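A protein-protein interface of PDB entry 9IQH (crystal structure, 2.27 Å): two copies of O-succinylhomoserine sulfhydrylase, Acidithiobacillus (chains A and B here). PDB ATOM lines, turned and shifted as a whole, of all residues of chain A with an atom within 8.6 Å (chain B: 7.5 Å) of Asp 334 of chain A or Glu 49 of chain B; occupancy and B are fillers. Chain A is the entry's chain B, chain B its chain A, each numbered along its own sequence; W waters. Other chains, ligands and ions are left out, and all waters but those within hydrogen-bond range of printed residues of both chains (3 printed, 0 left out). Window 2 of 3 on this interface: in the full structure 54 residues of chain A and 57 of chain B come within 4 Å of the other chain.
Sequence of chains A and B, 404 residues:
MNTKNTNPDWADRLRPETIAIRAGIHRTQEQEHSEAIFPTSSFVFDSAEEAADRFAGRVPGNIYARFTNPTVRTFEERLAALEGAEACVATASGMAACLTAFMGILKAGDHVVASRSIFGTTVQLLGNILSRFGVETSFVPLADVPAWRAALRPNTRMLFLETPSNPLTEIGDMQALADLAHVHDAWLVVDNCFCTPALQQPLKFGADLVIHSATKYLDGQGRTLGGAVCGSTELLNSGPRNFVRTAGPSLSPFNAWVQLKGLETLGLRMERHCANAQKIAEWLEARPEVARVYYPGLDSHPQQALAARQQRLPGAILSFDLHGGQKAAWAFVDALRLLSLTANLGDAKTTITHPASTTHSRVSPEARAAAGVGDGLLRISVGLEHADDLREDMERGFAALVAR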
ATOM      1  N   GLN A 326      -4.444  23.552 -23.558  1.00  0.00           N
ATOM      2  CA  GLN A 326      -4.914  23.305 -22.206  1.00  0.00           C
ATOM      3  C   GLN A 326      -5.249  21.837 -22.001  1.00  0.00           C
ATOM      4  O   GLN A 326      -4.987  21.277 -20.929  1.00  0.00           O
ATOM      5  CB  GLN A 326      -6.125  24.180 -21.913  1.00  0.00           C
ATOM      6  CG  GLN A 326      -6.746  23.905 -20.574  1.00  0.00           C
ATOM      7  CD  GLN A 326      -7.762  24.945 -20.215  1.00  0.00           C
ATOM      8  OE1 GLN A 326      -8.942  24.641 -20.063  1.00  0.00           O
ATOM      9  NE2 GLN A 326      -7.315  26.190 -20.086  1.00  0.00           N
ATOM     10  N   LYS A 327      -5.820  21.194 -23.023  1.00  0.00           N
ATOM     11  CA  LYS A 327      -6.204  19.794 -22.885  1.00  0.00           C
ATOM     12  C   LYS A 327      -4.992  18.924 -22.577  1.00  0.00           C
ATOM     13  O   LYS A 327      -5.061  18.023 -21.732  1.00  0.00           O
ATOM     14  CB  LYS A 327      -6.898  19.315 -24.160  1.00  0.00           C
ATOM     15  CG  LYS A 327      -8.166  18.492 -23.929  1.00  0.00           C
ATOM     16  CD  LYS A 327      -7.908  17.243 -23.088  1.00  0.00           C
ATOM     17  CE  LYS A 327      -8.554  17.350 -21.702  1.00  0.00           C
ATOM     18  NZ  LYS A 327      -7.559  17.479 -20.595  1.00  0.00           N
ATOM     19  N   ALA A 328      -3.873  19.174 -23.258  1.00  0.00           N
ATOM     20  CA  ALA A 328      -2.659  18.405 -23.004  1.00  0.00           C
ATOM     21  C   ALA A 328      -2.113  18.666 -21.604  1.00  0.00           C
ATOM     22  O   ALA A 328      -1.716  17.728 -20.903  1.00  0.00           O
ATOM     23  CB  ALA A 328      -1.608  18.732 -24.064  1.00  0.00           C
ATOM     24  N   ALA A 329      -2.091  19.931 -21.180  1.00  0.00           N
ATOM     25  CA  ALA A 329      -1.608  20.257 -19.842  1.00  0.00           C
ATOM     26  C   ALA A 329      -2.473  19.609 -18.767  1.00  0.00           C
ATOM     27  O   ALA A 329      -1.950  19.048 -17.795  1.00  0.00           O
ATOM     28  CB  ALA A 329      -1.567  21.773 -19.659  1.00  0.00           C
ATOM     29  N   TRP A 330      -3.802  19.658 -18.931  1.00  0.00           N
ATOM     30  CA  TRP A 330      -4.694  19.100 -17.921  1.00  0.00           C
ATOM     31  C   TRP A 330      -4.615  17.580 -17.892  1.00  0.00           C
ATOM     32  O   TRP A 330      -4.636  16.971 -16.815  1.00  0.00           O
ATOM     33  CB  TRP A 330      -6.128  19.566 -18.162  1.00  0.00           C
ATOM     34  CG  TRP A 330      -6.358  21.000 -17.793  1.00  0.00           C
ATOM     35  CD1 TRP A 330      -5.405  21.952 -17.562  1.00  0.00           C
ATOM     36  CD2 TRP A 330      -7.622  21.644 -17.592  1.00  0.00           C
ATOM     37  NE1 TRP A 330      -5.998  23.150 -17.240  1.00  0.00           N
ATOM     38  CE2 TRP A 330      -7.358  22.987 -17.247  1.00  0.00           C
ATOM     39  CE3 TRP A 330      -8.953  21.214 -17.671  1.00  0.00           C
ATOM     40  CZ2 TRP A 330      -8.377  23.907 -16.989  1.00  0.00           C
ATOM     41  CZ3 TRP A 330      -9.963  22.128 -17.410  1.00  0.00           C
ATOM     42  CH2 TRP A 330      -9.669  23.458 -17.072  1.00  0.00           C
ATOM     43  N   ALA A 331      -4.527  16.944 -19.060  1.00  0.00           N
ATOM     44  CA  ALA A 331      -4.304  15.504 -19.081  1.00  0.00           C
ATOM     45  C   ALA A 331      -2.993  15.156 -18.393  1.00  0.00           C
ATOM     46  O   ALA A 331      -2.887  14.124 -17.719  1.00  0.00           O
ATOM     47  CB  ALA A 331      -4.308  14.991 -20.521  1.00  0.00           C
ATOM     48  N   PHE A 332      -1.984  16.012 -18.552  1.00  0.00           N
ATOM     49  CA  PHE A 332      -0.686  15.770 -17.935  1.00  0.00           C
ATOM     50  C   PHE A 332      -0.778  15.806 -16.412  1.00  0.00           C
ATOM     51  O   PHE A 332      -0.329  14.876 -15.732  1.00  0.00           O
ATOM     52  CB  PHE A 332       0.321  16.802 -18.445  1.00  0.00           C
ATOM     53  CG  PHE A 332       1.717  16.599 -17.938  1.00  0.00           C
ATOM     54  CD1 PHE A 332       2.125  17.159 -16.734  1.00  0.00           C
ATOM     55  CD2 PHE A 332       2.632  15.867 -18.675  1.00  0.00           C
ATOM     56  CE1 PHE A 332       3.414  16.976 -16.263  1.00  0.00           C
ATOM     57  CE2 PHE A 332       3.922  15.679 -18.211  1.00  0.00           C
ATOM     58  CZ  PHE A 332       4.316  16.237 -17.003  1.00  0.00           C
ATOM     59  N   VAL A 333      -1.343  16.881 -15.851  1.00  0.00           N
ATOM     60  CA  VAL A 333      -1.310  16.997 -14.396  1.00  0.00           C
ATOM     61  C   VAL A 333      -2.267  16.002 -13.754  1.00  0.00           C
ATOM     62  O   VAL A 333      -1.979  15.475 -12.675  1.00  0.00           O
ATOM     63  CB  VAL A 333      -1.585  18.442 -13.920  1.00  0.00           C
ATOM     64  CG1 VAL A 333      -0.852  19.459 -14.783  1.00  0.00           C
ATOM     65  CG2 VAL A 333      -3.050  18.743 -13.857  1.00  0.00           C
ATOM     66  N   ASP A 334      -3.397  15.701 -14.409  1.00  0.00           N
ATOM     67  CA  ASP A 334      -4.389  14.818 -13.807  1.00  0.00           C
ATOM     68  C   ASP A 334      -3.872  13.399 -13.616  1.00  0.00           C
ATOM     69  O   ASP A 334      -4.438  12.652 -12.811  1.00  0.00           O
ATOM     70  CB  ASP A 334      -5.665  14.796 -14.651  1.00  0.00           C
ATOM     71  CG  ASP A 334      -6.491  16.064 -14.495  1.00  0.00           C
ATOM     72  OD1 ASP A 334      -6.079  16.953 -13.721  1.00  0.00           O
ATOM     73  OD2 ASP A 334      -7.553  16.175 -15.146  1.00  0.00           O
ATOM     74  N   ALA A 335      -2.821  13.006 -14.331  1.00  0.00           N
ATOM     75  CA  ALA A 335      -2.263  11.672 -14.176  1.00  0.00           C
ATOM     76  C   ALA A 335      -1.169  11.605 -13.117  1.00  0.00           C
ATOM     77  O   ALA A 335      -0.748  10.503 -12.751  1.00  0.00           O
ATOM     78  CB  ALA A 335      -1.712  11.176 -15.517  1.00  0.00           C
ATOM     79  N   LEU A 336      -0.706  12.745 -12.616  1.00  0.00           N
ATOM     80  CA  LEU A 336       0.332  12.752 -11.597  1.00  0.00           C
ATOM     81  C   LEU A 336      -0.223  12.240 -10.274  1.00  0.00           C
ATOM     82  O   LEU A 336      -1.352  12.558  -9.892  1.00  0.00           O
ATOM     83  CB  LEU A 336       0.888  14.164 -11.425  1.00  0.00           C
ATOM     84  CG  LEU A 336       1.359  14.856 -12.705  1.00  0.00           C
ATOM     85  CD1 LEU A 336       1.800  16.277 -12.421  1.00  0.00           C
ATOM     86  CD2 LEU A 336       2.483  14.068 -13.357  1.00  0.00           C
ATOM     87  N   ARG A 337       0.573  11.427  -9.581  1.00  0.00           N
ATOM     88  CA  ARG A 337       0.224  10.947  -8.252  1.00  0.00           C
ATOM     89  C   ARG A 337       1.160  11.437  -7.157  1.00  0.00           C
ATOM     90  O   ARG A 337       0.877  11.200  -5.976  1.00  0.00           O
ATOM     91  CB  ARG A 337       0.202   9.410  -8.211  1.00  0.00           C
ATOM     92  CG  ARG A 337      -0.630   8.744  -9.288  1.00  0.00           C
ATOM     93  CD  ARG A 337      -0.972   7.313  -8.883  1.00  0.00           C
ATOM     94  NE  ARG A 337      -1.486   6.529  -9.999  1.00  0.00           N
ATOM     95  CZ  ARG A 337      -0.765   5.665 -10.701  1.00  0.00           C
ATOM     96  NH1 ARG A 337       0.506   5.432 -10.415  1.00  0.00           N
ATOM     97  NH2 ARG A 337      -1.333   5.017 -11.713  1.00  0.00           N
ATOM     98  N   LEU A 338       2.263  12.097  -7.503  1.00  0.00           N
ATOM     99  CA  LEU A 338       3.247  12.541  -6.523  1.00  0.00           C
ATOM    100  C   LEU A 338       3.322  14.054  -6.401  1.00  0.00           C
ATOM    101  O   LEU A 338       3.200  14.587  -5.294  1.00  0.00           O
ATOM    102  CB  LEU A 338       4.628  11.982  -6.876  1.00  0.00           C
ATOM    103  CG  LEU A 338       5.753  12.303  -5.893  1.00  0.00           C
ATOM    104  CD1 LEU A 338       5.436  11.740  -4.517  1.00  0.00           C
ATOM    105  CD2 LEU A 338       7.074  11.755  -6.413  1.00  0.00           C
ATOM    106  N   LEU A 341      -0.573  19.397  -6.830  1.00  0.00           N
ATOM    107  CA  LEU A 341      -1.356  20.353  -7.608  1.00  0.00           C
ATOM    108  C   LEU A 341      -1.739  21.488  -6.677  1.00  0.00           C
ATOM    109  O   LEU A 341      -2.695  21.378  -5.909  1.00  0.00           O
ATOM    110  CB  LEU A 341      -2.602  19.704  -8.199  1.00  0.00           C
ATOM    111  CG  LEU A 341      -2.501  18.924  -9.506  1.00  0.00           C
ATOM    112  CD1 LEU A 341      -1.655  17.669  -9.335  1.00  0.00           C
ATOM    113  CD2 LEU A 341      -3.901  18.576 -10.001  1.00  0.00           C
ATOM    114  N   ILE A 352       3.109  21.792  -8.907  1.00  0.00           N
ATOM    115  CA  ILE A 352       2.868  22.096 -10.309  1.00  0.00           C
ATOM    116  C   ILE A 352       1.540  22.831 -10.400  1.00  0.00           C
ATOM    117  O   ILE A 352       0.619  22.597  -9.611  1.00  0.00           O
ATOM    118  CB  ILE A 352       2.893  20.824 -11.196  1.00  0.00           C
ATOM    119  CG1 ILE A 352       2.871  21.195 -12.680  1.00  0.00           C
ATOM    120  CG2 ILE A 352       1.752  19.875 -10.833  1.00  0.00           C
ATOM    121  CD1 ILE A 352       3.061  20.007 -13.592  1.00  0.00           C
ATOM    122  N   HIS A 354      -1.030  25.187 -13.524  1.00  0.00           N
ATOM    123  CA  HIS A 354      -1.269  25.579 -14.909  1.00  0.00           C
ATOM    124  C   HIS A 354      -1.665  27.046 -14.918  1.00  0.00           C
ATOM    125  O   HIS A 354      -2.827  27.374 -14.633  1.00  0.00           O
ATOM    126  CB  HIS A 354      -2.372  24.713 -15.526  1.00  0.00           C
ATOM    127  CG  HIS A 354      -2.733  25.087 -16.931  1.00  0.00           C
ATOM    128  ND1 HIS A 354      -3.915  25.723 -17.250  1.00  0.00           N
ATOM    129  CD2 HIS A 354      -2.079  24.900 -18.101  1.00  0.00           C
ATOM    130  CE1 HIS A 354      -3.969  25.917 -18.556  1.00  0.00           C
ATOM    131  NE2 HIS A 354      -2.865  25.430 -19.095  1.00  0.00           N
ATOM    132  N   SER A 357      -5.043  28.801 -16.424  1.00  0.00           N
ATOM    133  CA  SER A 357      -6.314  28.574 -15.753  1.00  0.00           C
ATOM    134  C   SER A 357      -6.281  28.819 -14.250  1.00  0.00           C
ATOM    135  O   SER A 357      -7.337  28.721 -13.613  1.00  0.00           O
ATOM    136  CB  SER A 357      -6.802  27.139 -16.003  1.00  0.00           C
ATOM    137  OG  SER A 357      -5.991  26.203 -15.311  1.00  0.00           O
ATOM    138  N   THR A 358      -5.115  29.071 -13.642  1.00  0.00           N
ATOM    139  CA  THR A 358      -5.089  29.351 -12.207  1.00  0.00           C
ATOM    140  C   THR A 358      -4.525  30.725 -11.866  1.00  0.00           C
ATOM    141  O   THR A 358      -5.303  31.644 -11.604  1.00  0.00           O
ATOM    142  CB  THR A 358      -4.283  28.257 -11.508  1.00  0.00           C
ATOM    143  OG1 THR A 358      -2.948  28.261 -12.034  1.00  0.00           O
ATOM    144  CG2 THR A 358      -4.916  26.885 -11.731  1.00  0.00           C
ATOM    145  N   LEU A 378       3.053  24.713 -18.208  1.00  0.00           N
ATOM    146  CA  LEU A 378       2.971  24.227 -16.838  1.00  0.00           C
ATOM    147  C   LEU A 378       4.181  24.734 -16.070  1.00  0.00           C
ATOM    148  O   LEU A 378       5.291  24.783 -16.611  1.00  0.00           O
ATOM    149  CB  LEU A 378       2.922  22.693 -16.789  1.00  0.00           C
ATOM    150  CG  LEU A 378       1.600  22.099 -17.270  1.00  0.00           C
ATOM    151  CD1 LEU A 378       1.708  20.596 -17.442  1.00  0.00           C
ATOM    152  CD2 LEU A 378       0.499  22.472 -16.291  1.00  0.00           C
ATOM    153  N   ASP A 393       7.077  10.217 -11.941  1.00  0.00           N
ATOM    154  CA  ASP A 393       5.723  10.747 -11.855  1.00  0.00           C
ATOM    155  C   ASP A 393       5.376  11.549 -13.098  1.00  0.00           C
ATOM    156  O   ASP A 393       4.260  11.444 -13.621  1.00  0.00           O
ATOM    157  CB  ASP A 393       5.556  11.596 -10.593  1.00  0.00           C
ATOM    158  CG  ASP A 393       4.096  11.897 -10.285  1.00  0.00           C
ATOM    159  OD1 ASP A 393       3.268  10.959 -10.328  1.00  0.00           O
ATOM    160  OD2 ASP A 393       3.778  13.069  -9.992  1.00  0.00           O
ATOM    161  N   ARG A 396       4.282   9.580 -15.964  1.00  0.00           N
ATOM    162  CA  ARG A 396       2.859   9.250 -15.951  1.00  0.00           C
ATOM    163  C   ARG A 396       2.043  10.326 -16.653  1.00  0.00           C
ATOM    164  O   ARG A 396       1.022  10.028 -17.282  1.00  0.00           O
ATOM    165  CB  ARG A 396       2.356   9.070 -14.519  1.00  0.00           C
ATOM    166  CG  ARG A 396       3.012   7.955 -13.730  1.00  0.00           C
ATOM    167  CD  ARG A 396       2.357   7.811 -12.356  1.00  0.00           C
ATOM    168  NE  ARG A 396       2.992   6.758 -11.574  1.00  0.00           N
ATOM    169  CZ  ARG A 396       3.950   6.958 -10.678  1.00  0.00           C
ATOM    170  NH1 ARG A 396       4.374   8.174 -10.376  1.00  0.00           N
ATOM    171  NH2 ARG A 396       4.497   5.908 -10.069  1.00  0.00           N
ATOM    172  N   GLY A 397       2.448  11.587 -16.518  1.00  0.00           N
ATOM    173  CA  GLY A 397       1.743  12.654 -17.209  1.00  0.00           C
ATOM    174  C   GLY A 397       1.939  12.596 -18.710  1.00  0.00           C
ATOM    175  O   GLY A 397       1.017  12.881 -19.479  1.00  0.00           O
ATOM    176  N   ALA A 400      -0.074   9.812 -20.284  1.00  0.00           N
ATOM    177  CA  ALA A 400      -1.482  10.159 -20.441  1.00  0.00           C
ATOM    178  C   ALA A 400      -1.755  10.974 -21.700  1.00  0.00           C
ATOM    179  O   ALA A 400      -2.923  11.143 -22.068  1.00  0.00           O
ATOM    180  CB  ALA A 400      -1.983  10.925 -19.216  1.00  0.00           C
ATOM    181  N   LEU A 401      -0.719  11.492 -22.355  1.00  0.00           N
ATOM    182  CA  LEU A 401      -0.895  12.168 -23.632  1.00  0.00           C
ATOM    183  C   LEU A 401      -1.135  11.198 -24.783  1.00  0.00           C
ATOM    184  O   LEU A 401      -1.496  11.639 -25.878  1.00  0.00           O
ATOM    185  CB  LEU A 401       0.326  13.040 -23.930  1.00  0.00           C
ATOM    186  CG  LEU A 401       0.287  14.495 -23.455  1.00  0.00           C
ATOM    187  CD1 LEU A 401      -0.686  14.689 -22.305  1.00  0.00           C
ATOM    188  CD2 LEU A 401       1.685  14.972 -23.066  1.00  0.00           C
ATOM    189  N   PHE B  45      -5.389  20.671  -4.970  1.00  0.00           N
ATOM    190  CA  PHE B  45      -6.586  20.406  -5.752  1.00  0.00           C
ATOM    191  C   PHE B  45      -6.586  18.960  -6.230  1.00  0.00           C
ATOM    192  O   PHE B  45      -5.530  18.338  -6.379  1.00  0.00           O
ATOM    193  CB  PHE B  45      -6.683  21.364  -6.944  1.00  0.00           C
ATOM    194  CG  PHE B  45      -6.498  22.803  -6.569  1.00  0.00           C
ATOM    195  CD1 PHE B  45      -7.445  23.457  -5.793  1.00  0.00           C
ATOM    196  CD2 PHE B  45      -5.369  23.502  -6.973  1.00  0.00           C
ATOM    197  CE1 PHE B  45      -7.275  24.782  -5.433  1.00  0.00           C
ATOM    198  CE2 PHE B  45      -5.198  24.833  -6.622  1.00  0.00           C
ATOM    199  CZ  PHE B  45      -6.153  25.472  -5.852  1.00  0.00           C
ATOM    200  N   ASP B  46      -7.791  18.419  -6.435  1.00  0.00           N
ATOM    201  CA  ASP B  46      -7.940  17.037  -6.880  1.00  0.00           C
ATOM    202  C   ASP B  46      -7.607  16.853  -8.353  1.00  0.00           C
ATOM    203  O   ASP B  46      -7.273  15.736  -8.767  1.00  0.00           O
ATOM    204  CB  ASP B  46      -9.369  16.548  -6.626  1.00  0.00           C
ATOM    205  CG  ASP B  46      -9.687  16.410  -5.147  1.00  0.00           C
ATOM    206  OD1 ASP B  46      -8.803  15.949  -4.389  1.00  0.00           O
ATOM    207  OD2 ASP B  46     -10.819  16.766  -4.743  1.00  0.00           O
ATOM    208  N   SER B  47      -7.694  17.919  -9.143  1.00  0.00           N
ATOM    209  CA  SER B  47      -7.507  17.851 -10.586  1.00  0.00           C
ATOM    210  C   SER B  47      -7.274  19.262 -11.097  1.00  0.00           C
ATOM    211  O   SER B  47      -7.538  20.246 -10.400  1.00  0.00           O
ATOM    212  CB  SER B  47      -8.724  17.231 -11.278  1.00  0.00           C
ATOM    213  OG  SER B  47      -9.867  18.050 -11.074  1.00  0.00           O
ATOM    214  N   ALA B  48      -6.789  19.348 -12.339  1.00  0.00           N
ATOM    215  CA  ALA B  48      -6.685  20.649 -12.992  1.00  0.00           C
ATOM    216  C   ALA B  48      -8.049  21.303 -13.101  1.00  0.00           C
ATOM    217  O   ALA B  48      -8.188  22.513 -12.878  1.00  0.00           O
ATOM    218  CB  ALA B  48      -6.058  20.505 -14.380  1.00  0.00           C
ATOM    219  N   GLU B  49      -9.071  20.508 -13.435  1.00  0.00           N
ATOM    220  CA  GLU B  49     -10.423  21.037 -13.553  1.00  0.00           C
ATOM    221  C   GLU B  49     -10.868  21.689 -12.250  1.00  0.00           C
ATOM    222  O   GLU B  49     -11.381  22.815 -12.244  1.00  0.00           O
ATOM    223  CB  GLU B  49     -11.382  19.912 -13.957  1.00  0.00           C
ATOM    224  CG  GLU B  49     -11.158  19.338 -15.361  1.00  0.00           C
ATOM    225  CD  GLU B  49      -9.992  18.353 -15.452  1.00  0.00           C
ATOM    226  OE1 GLU B  49      -9.269  18.161 -14.453  1.00  0.00           O
ATOM    227  OE2 GLU B  49      -9.804  17.768 -16.540  1.00  0.00           O
ATOM    228  N   GLU B  50     -10.658  20.997 -11.124  1.00  0.00           N
ATOM    229  CA  GLU B  50     -11.029  21.566  -9.832  1.00  0.00           C
ATOM    230  C   GLU B  50     -10.251  22.846  -9.553  1.00  0.00           C
ATOM    231  O   GLU B  50     -10.819  23.832  -9.070  1.00  0.00           O
ATOM    232  CB  GLU B  50     -10.800  20.545  -8.714  1.00  0.00           C
ATOM    233  CG  GLU B  50     -11.121  21.087  -7.327  1.00  0.00           C
ATOM    234  CD  GLU B  50     -11.062  20.025  -6.249  1.00  0.00           C
ATOM    235  OE1 GLU B  50      -9.945  19.695  -5.795  1.00  0.00           O
ATOM    236  OE2 GLU B  50     -12.136  19.517  -5.856  1.00  0.00           O
ATOM    237  N   ALA B  51      -8.952  22.854  -9.869  1.00  0.00           N
ATOM    238  CA  ALA B  51      -8.148  24.056  -9.666  1.00  0.00           C
ATOM    239  C   ALA B  51      -8.701  25.224 -10.467  1.00  0.00           C
ATOM    240  O   ALA B  51      -8.794  26.349  -9.959  1.00  0.00           O
ATOM    241  CB  ALA B  51      -6.692  23.795 -10.060  1.00  0.00           C
ATOM    242  N   ALA B  52      -9.071  24.974 -11.724  1.00  0.00           N
ATOM    243  CA  ALA B  52      -9.628  26.032 -12.556  1.00  0.00           C
ATOM    244  C   ALA B  52     -10.958  26.527 -12.003  1.00  0.00           C
ATOM    245  O   ALA B  52     -11.193  27.739 -11.931  1.00  0.00           O
ATOM    246  CB  ALA B  52      -9.784  25.533 -13.995  1.00  0.00           C
ATOM    247  N   ASP B  53     -11.833  25.603 -11.591  1.00  0.00           N
ATOM    248  CA  ASP B  53     -13.130  25.995 -11.045  1.00  0.00           C
ATOM    249  C   ASP B  53     -12.968  26.838  -9.791  1.00  0.00           C
ATOM    250  O   ASP B  53     -13.618  27.879  -9.637  1.00  0.00           O
ATOM    251  CB  ASP B  53     -13.967  24.756 -10.732  1.00  0.00           C
ATOM    252  CG  ASP B  53     -14.421  24.038 -11.972  1.00  0.00           C
ATOM    253  OD1 ASP B  53     -14.550  24.698 -13.025  1.00  0.00           O
ATOM    254  OD2 ASP B  53     -14.645  22.812 -11.890  1.00  0.00           O
ATOM    255  N   ARG B  54     -12.105  26.397  -8.875  1.00  0.00           N
ATOM    256  CA  ARG B  54     -11.913  27.136  -7.634  1.00  0.00           C
ATOM    257  C   ARG B  54     -11.311  28.514  -7.900  1.00  0.00           C
ATOM    258  O   ARG B  54     -11.731  29.510  -7.302  1.00  0.00           O
ATOM    259  CB  ARG B  54     -11.045  26.320  -6.676  1.00  0.00           C
ATOM    260  CG  ARG B  54     -11.277  26.644  -5.217  1.00  0.00           C
ATOM    261  CD  ARG B  54     -10.691  25.575  -4.324  1.00  0.00           C
ATOM    262  NE  ARG B  54     -11.486  24.355  -4.340  1.00  0.00           N
ATOM    263  CZ  ARG B  54     -11.181  23.261  -3.655  1.00  0.00           C
ATOM    264  NH1 ARG B  54     -10.095  23.202  -2.899  1.00  0.00           N
ATOM    265  NH2 ARG B  54     -11.981  22.201  -3.732  1.00  0.00           N
ATOM    266  N   PHE B  55     -10.338  28.596  -8.813  1.00  0.00           N
ATOM    267  CA  PHE B  55      -9.791  29.900  -9.172  1.00  0.00           C
ATOM    268  C   PHE B  55     -10.825  30.773  -9.873  1.00  0.00           C
ATOM    269  O   PHE B  55     -10.778  32.003  -9.753  1.00  0.00           O
ATOM    270  CB  PHE B  55      -8.553  29.732 -10.054  1.00  0.00           C
ATOM    271  CG  PHE B  55      -7.264  29.766  -9.292  1.00  0.00           C
ATOM    272  CD1 PHE B  55      -6.637  30.973  -9.021  1.00  0.00           C
ATOM    273  CD2 PHE B  55      -6.681  28.596  -8.832  1.00  0.00           C
ATOM    274  CE1 PHE B  55      -5.450  31.018  -8.316  1.00  0.00           C
ATOM    275  CE2 PHE B  55      -5.497  28.632  -8.121  1.00  0.00           C
ATOM    276  CZ  PHE B  55      -4.880  29.846  -7.862  1.00  0.00           C
ATOM    277  N   ARG B  58     -16.268  29.145  -9.478  1.00  0.00           N
ATOM    278  CA  ARG B  58     -17.416  28.294  -9.775  1.00  0.00           C
ATOM    279  C   ARG B  58     -17.706  27.303  -8.659  1.00  0.00           C
ATOM    280  O   ARG B  58     -18.850  26.864  -8.510  1.00  0.00           O
ATOM    281  CB  ARG B  58     -17.196  27.544 -11.085  1.00  0.00           C
ATOM    282  CG  ARG B  58     -17.315  28.421 -12.311  1.00  0.00           C
ATOM    283  CD  ARG B  58     -17.194  27.593 -13.570  1.00  0.00           C
ATOM    284  NE  ARG B  58     -15.840  27.095 -13.778  1.00  0.00           N
ATOM    285  CZ  ARG B  58     -14.903  27.744 -14.457  1.00  0.00           C
ATOM    286  NH1 ARG B  58     -15.124  28.950 -14.959  1.00  0.00           N
ATOM    287  NH2 ARG B  58     -13.718  27.168 -14.641  1.00  0.00           N
ATOM    288  N   VAL B  59     -16.695  26.927  -7.886  1.00  0.00           N
ATOM    289  CA  VAL B  59     -16.894  26.077  -6.718  1.00  0.00           C
ATOM    290  C   VAL B  59     -16.268  26.781  -5.520  1.00  0.00           C
ATOM    291  O   VAL B  59     -15.308  27.549  -5.681  1.00  0.00           O
ATOM    292  CB  VAL B  59     -16.294  24.673  -6.923  1.00  0.00           C
ATOM    293  CG1 VAL B  59     -16.959  23.959  -8.095  1.00  0.00           C
ATOM    294  CG2 VAL B  59     -14.796  24.760  -7.135  1.00  0.00           C
HETATM  295  O   HOH W   1      -5.680  23.960 -13.616  1.00  0.00           O
HETATM  296  O   HOH W   2      -7.941  16.703 -18.079  1.00  0.00           O
HETATM  297  O   HOH W   3     -10.066  29.071 -13.758  1.00  0.00           O
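The backbone carbonyl oxygen (O) of Leu 341 of chain A lies within hydrogen-bond range of the backbone NH (N) of Phe 45 of chain B (2.9 Å). N of Ala 48 of chain B lies within hydrogen-bond range of OD1 of Asp 334 of chain A (2.9 Å). The side-chain carboxylate (OE1) of Glu 49 of chain B lies close to the side-chain carboxylate (OD2) of Asp 334 of chain A (2.7 Å).
OE1 of Glu 49 of chain B sits close to OG of Ser 47 of chain B (3.4 Å). The side-chain hydroxyl (OG) of Ser 47 of chain B sits at hydrogen-bond distance from the backbone NH (N) of Glu 50 of chain B, at 3.1 Å. The indole nitrogen (NE1) of Trp 330 of chain A sits at hydrogen-bond distance from a ring nitrogen (ND1) of His 354 of chain A, 3.3 Å away. The side-chain hydroxyl of Ser 357 of chain A is in hydrogen-bond range of a ring nitrogen (ND1) of His 354 of chain A (2.9 Å). OG1 of Thr 358 of chain A sits at hydrogen-bond distance from O of His 354 of chain A (2.7 Å).
Among the printed residues, merely in contact across the chains: Trp 330 of chain A with Ala 48 of chain B, Trp 330 of chain A with Glu 49 of chain B, Trp 330 of chain A with Ala 52 of chain B, Val 333 of chain A with Ala 48 of chain B, Asp 334 of chain A with Ser 47 of chain B, Leu 341 of chain A with Ser 47 of chain B, Leu 341 of chain A with Ala 48 of chain B, Ser 357 of chain A with Ala 52 of chain B, Ser 357 of chain A with Phe 55 of chain B, Thr 358 of chain A with Ala 51 of chain B and Thr 358 of chain A with Phe 55 of chain B.
Of the printed residues of chain A, Glu 49 of chain B touches Trp 330 (3.7 Å) and Asp 334 (2.7 Å). Of the printed residues of chain B, Leu 341 of chain A touches Phe 45 (2.9 Å), Ser 47 (3.6 Å) and Ala 48 (3.8 Å). Of the printed residues of chain B, Ser 357 of chain A touches Ala 52 (3.7 Å) and Phe 55 (3.9 Å). Printed residues of chain A within 4 Å of Phe 55 of chain B: Ser 357 (3.9 Å) and Thr 358 (3.0 Å). Printed residues of chain B within 4 Å of Thr 358 of chain A: Ala 51 (3.9 Å) and Phe 55 (3.0 Å). Asp 393 of chain A touches none of the printed residues of chain B.
Of the 24 printed residues of chain A, 6 touch a printed residue of chain B. Hydrophobic or aromatic side chains of chain A within 4 Å of the printed part of chain B: Trp 330, Val 333 and Leu 341. Printed residues of chain B that touch a printed residue of chain A: Phe 45, Ser 47, Ala 48, Glu 49, Ala 51, Ala 52 and Phe 55. Among the printed residues, no Asp or Glu carboxylate lies within 4 Å of a Lys or Arg side-chain nitrogen of the other chain.
No position is printed for both chains.
Water W3 bridges O of Ala 52 of chain B (2.5 Å) and O of Ser 357 of chain A (2.8 Å). Water W2 lies within hydrogen-bond range of OE2 of Glu 49 of chain B (2.6 Å), NZ of Lys 327 of chain A (2.7 Å) and OD2 of Asp 334 of chain A (3.0 Å). Water W1 bridges OG of Ser 357 of chain A and O of Ala 48 of chain B.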
